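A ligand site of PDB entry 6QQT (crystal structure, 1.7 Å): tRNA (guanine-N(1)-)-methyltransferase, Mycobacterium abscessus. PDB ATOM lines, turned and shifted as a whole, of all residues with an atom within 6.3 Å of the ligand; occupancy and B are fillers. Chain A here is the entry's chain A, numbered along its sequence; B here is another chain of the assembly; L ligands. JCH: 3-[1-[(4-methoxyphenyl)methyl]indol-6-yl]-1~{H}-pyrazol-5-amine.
The backbone carbonyl oxygen (O) of Ile 135 is in hydrogen-bond range of the side-chain hydroxyl (OH) of Tyr 138. The backbone NH (N) of Thr 86 lies within hydrogen-bond range of the backbone carbonyl oxygen (O) of Val 133, 2.9 Å away. The side-chain hydroxyl (OG) of Ser 134 lies within hydrogen-bond range of the backbone carbonyl oxygen (O) of Gly 136, at 3.0 Å. OE1 of Glu 144 is in salt-bridge range of NE of Arg 112 (2.9 Å). N of Ala 88 sits close to OG1 of Thr 86 (3.0 Å). The backbone NH (N) of Gly 143 lies within hydrogen-bond range of the backbone carbonyl oxygen (O) of Gly 111, 2.9 Å away. The side-chain amide oxygen (OD1) of Asn 141 is in hydrogen-bond range of the guanidinium group (NE) of Arg 156 of chain B (3.1 Å).
A nitrogen (N01) of the ligand sits close to the backbone NH (N) of Ile 135 (3.1 Å). Pro 85 touches the ligand (O to C08, 3.3 Å). CA of Thr 86 touches C07 of the ligand (3.6 Å). CD of Pro 87 touches C06 of the ligand, 3.4 Å away. Gly 111 touches the ligand. C of Arg 112 touches C21 of the ligand, 3.7 Å away. O of Tyr 113 touches C21 of the ligand, 3.3 Å away. O of Glu 114 touches C15 of the ligand (3.6 Å). Val 139 touches the ligand (CG1 to C20, 3.4 Å). Asn 141 touches the ligand. CA of Gly 142 touches C09 of the ligand (3.5 Å). N of Gly 143 touches C08 of the ligand, at 3.5 Å. CG of Glu 182 of chain B touches O17 of the ligand (3.2 Å). Hydrophobic or aromatic side chains that line the ligand: Pro 85, Pro 87, Ile 135, Val 139 and Leu 140. Of the 26 residues printed, 17 come within 4 Å of the ligand. The nearest printed residue that does not touch the ligand is Gly 115 (4.1 Å).
N01 of the ligand sits at hydrogen-bond distance from OG of Ser 134 (3.0 Å). A nitrogen (N04) of the ligand is in hydrogen-bond range of the backbone NH of Leu 140, 3.0 Å away. A nitrogen (N01) of the ligand sits at hydrogen-bond distance from the backbone carbonyl oxygen (O) of Gly 136, at 3.1 Å. The backbone carbonyl oxygen of Tyr 138 sits at hydrogen-bond distance from a nitrogen (N03) of the ligand, at 2.7 Å.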
ATOM      1  N   PRO A  85       3.721  -3.642  25.879  1.00  0.00           N
ATOM      2  CA  PRO A  85       3.121  -4.879  25.348  1.00  0.00           C
ATOM      3  C   PRO A  85       4.132  -5.701  24.559  1.00  0.00           C
ATOM      4  O   PRO A  85       4.941  -5.156  23.807  1.00  0.00           O
ATOM      5  CB  PRO A  85       1.985  -4.364  24.450  1.00  0.00           C
ATOM      6  CG  PRO A  85       1.603  -3.035  25.082  1.00  0.00           C
ATOM      7  CD  PRO A  85       2.932  -2.446  25.535  1.00  0.00           C
ATOM      8  N   THR A  86       4.085  -7.011  24.732  1.00  0.00           N
ATOM      9  CA  THR A  86       4.968  -7.925  23.988  1.00  0.00           C
ATOM     10  C   THR A  86       4.433  -9.331  24.137  1.00  0.00           C
ATOM     11  O   THR A  86       3.916  -9.697  25.180  1.00  0.00           O
ATOM     12  CB  THR A  86       6.432  -7.850  24.488  1.00  0.00           C
ATOM     13  OG1 THR A  86       7.154  -9.003  24.011  1.00  0.00           O
ATOM     14  CG2 THR A  86       6.507  -7.785  25.996  1.00  0.00           C
ATOM     15  N   PRO A  87       4.541 -10.130  23.063  1.00  0.00           N
ATOM     16  CA  PRO A  87       4.116 -11.539  23.130  1.00  0.00           C
ATOM     17  C   PRO A  87       4.914 -12.318  24.171  1.00  0.00           C
ATOM     18  O   PRO A  87       4.439 -13.362  24.633  1.00  0.00           O
ATOM     19  CB  PRO A  87       4.393 -12.067  21.723  1.00  0.00           C
ATOM     20  CG  PRO A  87       4.573 -10.894  20.866  1.00  0.00           C
ATOM     21  CD  PRO A  87       5.075  -9.771  21.745  1.00  0.00           C
ATOM     22  N   ALA A  88       6.081 -11.798  24.544  1.00  0.00           N
ATOM     23  CA  ALA A  88       6.945 -12.459  25.522  1.00  0.00           C
ATOM     24  C   ALA A  88       6.775 -11.892  26.922  1.00  0.00           C
ATOM     25  O   ALA A  88       7.609 -12.123  27.797  1.00  0.00           O
ATOM     26  CB  ALA A  88       8.411 -12.363  25.083  1.00  0.00           C
ATOM     27  N   CYS A 110       4.143   1.208  22.434  1.00  0.00           N
ATOM     28  CA  CYS A 110       3.654   0.264  21.449  1.00  0.00           C
ATOM     29  C   CYS A 110       4.680  -0.046  20.394  1.00  0.00           C
ATOM     30  O   CYS A 110       5.042   0.824  19.603  1.00  0.00           O
ATOM     31  CB  CYS A 110       2.395   0.815  20.770  1.00  0.00           C
ATOM     32  SG  CYS A 110       1.005   1.061  21.881  1.00  0.00           S
ATOM     33  N   GLY A 111       5.160  -1.291  20.376  1.00  0.00           N
ATOM     34  CA  GLY A 111       6.066  -1.723  19.332  1.00  0.00           C
ATOM     35  C   GLY A 111       5.374  -2.162  18.049  1.00  0.00           C
ATOM     36  O   GLY A 111       4.152  -2.378  17.999  1.00  0.00           O
ATOM     37  N   ARG A 112       6.186  -2.277  17.005  1.00  0.00           N
ATOM     38  CA  ARG A 112       5.795  -2.902  15.736  1.00  0.00           C
ATOM     39  C   ARG A 112       6.980  -3.742  15.255  1.00  0.00           C
ATOM     40  O   ARG A 112       7.960  -3.900  15.988  1.00  0.00           O
ATOM     41  CB  ARG A 112       5.395  -1.847  14.706  1.00  0.00           C
ATOM     42  CG  ARG A 112       3.987  -1.261  14.894  1.00  0.00           C
ATOM     43  CD  ARG A 112       2.963  -2.109  14.128  1.00  0.00           C
ATOM     44  NE  ARG A 112       1.602  -1.965  14.664  1.00  0.00           N
ATOM     45  CZ  ARG A 112       0.526  -2.482  14.090  1.00  0.00           C
ATOM     46  NH1 ARG A 112       0.640  -3.128  12.934  1.00  0.00           N
ATOM     47  NH2 ARG A 112      -0.672  -2.309  14.641  1.00  0.00           N
ATOM     48  N   TYR A 113       6.896  -4.286  14.040  1.00  0.00           N
ATOM     49  CA  TYR A 113       7.947  -5.161  13.508  1.00  0.00           C
ATOM     50  C   TYR A 113       8.205  -6.317  14.458  1.00  0.00           C
ATOM     51  O   TYR A 113       7.267  -6.986  14.888  1.00  0.00           O
ATOM     52  CB  TYR A 113       9.230  -4.361  13.234  1.00  0.00           C
ATOM     53  CG  TYR A 113       8.971  -3.139  12.385  1.00  0.00           C
ATOM     54  CD1 TYR A 113       8.966  -3.221  10.998  1.00  0.00           C
ATOM     55  CD2 TYR A 113       8.723  -1.896  12.968  1.00  0.00           C
ATOM     56  CE1 TYR A 113       8.732  -2.111  10.218  1.00  0.00           C
ATOM     57  CE2 TYR A 113       8.478  -0.780  12.195  1.00  0.00           C
ATOM     58  CZ  TYR A 113       8.483  -0.889  10.815  1.00  0.00           C
ATOM     59  OH  TYR A 113       8.247   0.224  10.045  1.00  0.00           O
ATOM     60  N   GLU A 114       9.467  -6.567  14.807  1.00  0.00           N
ATOM     61  CA  GLU A 114       9.791  -7.682  15.699  1.00  0.00           C
ATOM     62  C   GLU A 114       9.881  -7.233  17.153  1.00  0.00           C
ATOM     63  O   GLU A 114      10.148  -8.040  18.023  1.00  0.00           O
ATOM     64  CB  GLU A 114      11.102  -8.361  15.283  1.00  0.00           C
ATOM     65  N   GLY A 115       9.629  -5.949  17.415  1.00  0.00           N
ATOM     66  CA  GLY A 115       9.652  -5.449  18.783  1.00  0.00           C
ATOM     67  C   GLY A 115      10.673  -4.349  18.968  1.00  0.00           C
ATOM     68  O   GLY A 115      11.245  -3.878  17.997  1.00  0.00           O
ATOM     69  N   ILE A 116      10.896  -3.940  20.206  1.00  0.00           N
ATOM     70  CA  ILE A 116      11.791  -2.834  20.531  1.00  0.00           C
ATOM     71  C   ILE A 116      13.124  -3.370  21.046  1.00  0.00           C
ATOM     72  O   ILE A 116      13.119  -4.345  21.804  1.00  0.00           O
ATOM     73  CB  ILE A 116      11.160  -1.906  21.591  1.00  0.00           C
ATOM     74  CG1 ILE A 116       9.756  -1.475  21.136  1.00  0.00           C
ATOM     75  CG2 ILE A 116      12.056  -0.706  21.887  1.00  0.00           C
ATOM     76  CD1 ILE A 116       8.987  -0.694  22.199  1.00  0.00           C
ATOM     77  N   VAL A 133       4.291  -6.906  29.239  1.00  0.00           N
ATOM     78  CA  VAL A 133       3.114  -7.751  29.429  1.00  0.00           C
ATOM     79  C   VAL A 133       2.503  -8.248  28.132  1.00  0.00           C
ATOM     80  O   VAL A 133       2.523  -7.553  27.112  1.00  0.00           O
ATOM     81  CB  VAL A 133       1.976  -7.014  30.231  1.00  0.00           C
ATOM     82  CG1 VAL A 133       2.416  -6.753  31.677  1.00  0.00           C
ATOM     83  CG2 VAL A 133       1.552  -5.712  29.531  1.00  0.00           C
ATOM     84  N   SER A 134       1.945  -9.454  28.215  1.00  0.00           N
ATOM     85  CA  SER A 134       1.193 -10.075  27.124  1.00  0.00           C
ATOM     86  C   SER A 134      -0.288 -10.063  27.497  1.00  0.00           C
ATOM     87  O   SER A 134      -0.642 -10.277  28.655  1.00  0.00           O
ATOM     88  CB  SER A 134       1.654 -11.513  26.892  1.00  0.00           C
ATOM     89  OG  SER A 134       0.730 -12.243  26.101  1.00  0.00           O
ATOM     90  N   ILE A 135      -1.175  -9.842  26.520  1.00  0.00           N
ATOM     91  CA  ILE A 135      -2.611  -9.866  26.836  1.00  0.00           C
ATOM     92  C   ILE A 135      -3.283 -11.203  26.498  1.00  0.00           C
ATOM     93  O   ILE A 135      -4.496 -11.361  26.698  1.00  0.00           O
ATOM     94  CB  ILE A 135      -3.390  -8.728  26.131  1.00  0.00           C
ATOM     95  CG1 ILE A 135      -3.289  -8.840  24.605  1.00  0.00           C
ATOM     96  CG2 ILE A 135      -2.952  -7.355  26.645  1.00  0.00           C
ATOM     97  CD1 ILE A 135      -4.415  -8.058  23.863  1.00  0.00           C
ATOM     98  N   GLY A 136      -2.507 -12.143  25.978  1.00  0.00           N
ATOM     99  CA  GLY A 136      -3.046 -13.465  25.703  1.00  0.00           C
ATOM    100  C   GLY A 136      -2.115 -14.273  24.823  1.00  0.00           C
ATOM    101  O   GLY A 136      -1.121 -13.736  24.317  1.00  0.00           O
ATOM    102  N   ASP A 137      -2.448 -15.543  24.641  1.00  0.00           N
ATOM    103  CA  ASP A 137      -1.549 -16.449  23.931  1.00  0.00           C
ATOM    104  C   ASP A 137      -1.852 -16.490  22.436  1.00  0.00           C
ATOM    105  O   ASP A 137      -2.193 -17.535  21.895  1.00  0.00           O
ATOM    106  CB  ASP A 137      -1.625 -17.838  24.540  1.00  0.00           C
ATOM    107  CG  ASP A 137      -0.958 -17.895  25.908  1.00  0.00           C
ATOM    108  OD1 ASP A 137      -0.181 -16.960  26.203  1.00  0.00           O
ATOM    109  OD2 ASP A 137      -1.191 -18.858  26.660  1.00  0.00           O
ATOM    110  N   TYR A 138      -1.709 -15.330  21.813  1.00  0.00           N
ATOM    111  CA  TYR A 138      -1.838 -15.177  20.375  1.00  0.00           C
ATOM    112  C   TYR A 138      -0.876 -14.049  20.013  1.00  0.00           C
ATOM    113  O   TYR A 138      -0.460 -13.285  20.875  1.00  0.00           O
ATOM    114  CB  TYR A 138      -3.250 -14.826  19.955  1.00  0.00           C
ATOM    115  CG  TYR A 138      -3.910 -13.895  20.926  1.00  0.00           C
ATOM    116  CD1 TYR A 138      -3.601 -12.525  20.937  1.00  0.00           C
ATOM    117  CD2 TYR A 138      -4.795 -14.372  21.888  1.00  0.00           C
ATOM    118  CE1 TYR A 138      -4.164 -11.673  21.880  1.00  0.00           C
ATOM    119  CE2 TYR A 138      -5.378 -13.524  22.818  1.00  0.00           C
ATOM    120  CZ  TYR A 138      -5.071 -12.178  22.802  1.00  0.00           C
ATOM    121  OH  TYR A 138      -5.628 -11.332  23.717  1.00  0.00           O
ATOM    122  N   VAL A 139      -0.587 -13.941  18.728  1.00  0.00           N
ATOM    123  CA  VAL A 139       0.390 -12.966  18.244  1.00  0.00           C
ATOM    124  C   VAL A 139      -0.316 -11.869  17.458  1.00  0.00           C
ATOM    125  O   VAL A 139      -1.076 -12.148  16.534  1.00  0.00           O
ATOM    126  CB  VAL A 139       1.439 -13.650  17.362  1.00  0.00           C
ATOM    127  CG1 VAL A 139       2.451 -12.626  16.864  1.00  0.00           C
ATOM    128  CG2 VAL A 139       2.136 -14.757  18.127  1.00  0.00           C
ATOM    129  N   LEU A 140      -0.056 -10.622  17.827  1.00  0.00           N
ATOM    130  CA  LEU A 140      -0.594  -9.469  17.115  1.00  0.00           C
ATOM    131  C   LEU A 140       0.479  -8.896  16.180  1.00  0.00           C
ATOM    132  O   LEU A 140       1.607  -9.393  16.169  1.00  0.00           O
ATOM    133  CB  LEU A 140      -1.052  -8.397  18.086  1.00  0.00           C
ATOM    134  CG  LEU A 140      -2.104  -8.825  19.120  1.00  0.00           C
ATOM    135  CD1 LEU A 140      -2.239  -7.781  20.212  1.00  0.00           C
ATOM    136  CD2 LEU A 140      -3.448  -9.061  18.437  1.00  0.00           C
ATOM    137  N   ASN A 141       0.143  -7.860  15.416  1.00  0.00           N
ATOM    138  CA  ASN A 141       1.130  -7.209  14.542  1.00  0.00           C
ATOM    139  C   ASN A 141       1.949  -6.164  15.291  1.00  0.00           C
ATOM    140  O   ASN A 141       3.020  -5.730  14.841  1.00  0.00           O
ATOM    141  CB  ASN A 141       0.452  -6.533  13.359  1.00  0.00           C
ATOM    142  CG  ASN A 141       0.079  -7.506  12.277  1.00  0.00           C
ATOM    143  OD1 ASN A 141       0.755  -8.529  12.077  1.00  0.00           O
ATOM    144  ND2 ASN A 141      -0.994  -7.206  11.560  1.00  0.00           N
ATOM    145  N   GLY A 142       1.443  -5.741  16.446  1.00  0.00           N
ATOM    146  CA  GLY A 142       2.092  -4.696  17.203  1.00  0.00           C
ATOM    147  C   GLY A 142       1.353  -4.430  18.490  1.00  0.00           C
ATOM    148  O   GLY A 142       0.357  -5.112  18.787  1.00  0.00           O
ATOM    149  N   GLY A 143       1.811  -3.445  19.243  1.00  0.00           N
ATOM    150  CA  GLY A 143       1.290  -3.236  20.584  1.00  0.00           C
ATOM    151  C   GLY A 143      -0.016  -2.472  20.704  1.00  0.00           C
ATOM    152  O   GLY A 143      -0.601  -2.430  21.786  1.00  0.00           O
ATOM    153  N   GLU A 144      -0.482  -1.867  19.617  1.00  0.00           N
ATOM    154  CA  GLU A 144      -1.631  -0.957  19.707  1.00  0.00           C
ATOM    155  C   GLU A 144      -2.919  -1.632  20.184  1.00  0.00           C
ATOM    156  O   GLU A 144      -3.635  -1.086  21.034  1.00  0.00           O
ATOM    157  CB  GLU A 144      -1.883  -0.279  18.357  1.00  0.00           C
ATOM    158  CG  GLU A 144      -0.815   0.760  18.002  1.00  0.00           C
ATOM    159  CD  GLU A 144       0.475   0.150  17.443  1.00  0.00           C
ATOM    160  OE1 GLU A 144       0.531  -1.062  17.149  1.00  0.00           O
ATOM    161  OE2 GLU A 144       1.444   0.927  17.299  1.00  0.00           O
ATOM    162  N   ALA A 146      -3.169  -4.283  21.939  1.00  0.00           N
ATOM    163  CA  ALA A 146      -2.923  -4.578  23.346  1.00  0.00           C
ATOM    164  C   ALA A 146      -3.109  -3.340  24.222  1.00  0.00           C
ATOM    165  O   ALA A 146      -3.667  -3.418  25.313  1.00  0.00           O
ATOM    166  CB  ALA A 146      -1.520  -5.161  23.541  1.00  0.00           C
ATOM    167  N   ARG B 156      -3.401 -11.718  10.050  1.00  0.00           N
ATOM    168  CA  ARG B 156      -1.972 -11.810   9.746  1.00  0.00           C
ATOM    169  C   ARG B 156      -1.566 -13.242   9.357  1.00  0.00           C
ATOM    170  O   ARG B 156      -0.460 -13.467   8.860  1.00  0.00           O
ATOM    171  CB  ARG B 156      -1.156 -11.294  10.933  1.00  0.00           C
ATOM    172  CG  ARG B 156      -1.214 -12.157  12.167  1.00  0.00           C
ATOM    173  CD  ARG B 156      -0.538 -11.471  13.344  1.00  0.00           C
ATOM    174  NE  ARG B 156       0.922 -11.424  13.215  1.00  0.00           N
ATOM    175  CZ  ARG B 156       1.720 -12.469  13.386  1.00  0.00           C
ATOM    176  NH1 ARG B 156       1.215 -13.666  13.654  1.00  0.00           N
ATOM    177  NH2 ARG B 156       3.037 -12.325  13.271  1.00  0.00           N
ATOM    178  N   GLU B 182       9.709 -15.576  22.767  1.00  0.00           N
ATOM    179  CA  GLU B 182      10.782 -14.925  22.025  1.00  0.00           C
ATOM    180  C   GLU B 182      11.723 -14.226  22.992  1.00  0.00           C
ATOM    181  O   GLU B 182      11.282 -13.593  23.941  1.00  0.00           O
ATOM    182  CB  GLU B 182      10.218 -13.926  21.026  1.00  0.00           C
ATOM    183  CG  GLU B 182       9.580 -14.567  19.816  1.00  0.00           C
ATOM    184  CD  GLU B 182      10.561 -15.409  19.025  1.00  0.00           C
ATOM    185  OE1 GLU B 182      11.706 -14.958  18.815  1.00  0.00           O
ATOM    186  OE2 GLU B 182      10.183 -16.530  18.627  1.00  0.00           O
HETATM  187  C10 JCH L   1       4.004  -7.226  18.817  1.00  0.00           C
HETATM  188  C13 JCH L   1       5.530  -9.458  16.918  1.00  0.00           C
HETATM  189  C15 JCH L   1       7.509 -10.479  17.970  1.00  0.00           C
HETATM  190  C20 JCH L   1       5.222 -10.650  16.362  1.00  0.00           C
HETATM  191  C21 JCH L   1       5.501  -6.163  17.554  1.00  0.00           C
HETATM  192  C22 JCH L   1       5.302  -5.425  18.706  1.00  0.00           C
HETATM  193  C24 JCH L   1       1.217  -9.024  22.480  1.00  0.00           C
HETATM  194  N01 JCH L   1      -0.249 -10.774  23.711  1.00  0.00           N
HETATM  195  C02 JCH L   1       0.372 -10.204  22.553  1.00  0.00           C
HETATM  196  N03 JCH L   1       0.298 -10.712  21.312  1.00  0.00           N
HETATM  197  N04 JCH L   1       1.024  -9.930  20.485  1.00  0.00           N
HETATM  198  C05 JCH L   1       1.545  -8.878  21.195  1.00  0.00           C
HETATM  199  C06 JCH L   1       2.475  -7.860  20.620  1.00  0.00           C
HETATM  200  C07 JCH L   1       2.814  -6.728  21.340  1.00  0.00           C
HETATM  201  C08 JCH L   1       3.763  -5.835  20.795  1.00  0.00           C
HETATM  202  C09 JCH L   1       4.342  -6.106  19.519  1.00  0.00           C
HETATM  203  N11 JCH L   1       4.717  -7.237  17.639  1.00  0.00           N
HETATM  204  C12 JCH L   1       4.601  -8.292  16.635  1.00  0.00           C
HETATM  205  C14 JCH L   1       6.659  -9.331  17.737  1.00  0.00           C
HETATM  206  C16 JCH L   1       7.201 -11.685  17.395  1.00  0.00           C
HETATM  207  O17 JCH L   1       8.020 -12.809  17.617  1.00  0.00           O
HETATM  208  C18 JCH L   1       9.114 -12.906  16.666  1.00  0.00           C
HETATM  209  C19 JCH L   1       6.082 -11.802  16.597  1.00  0.00           C
HETATM  210  C23 JCH L   1       3.053  -8.151  19.359  1.00  0.00           C
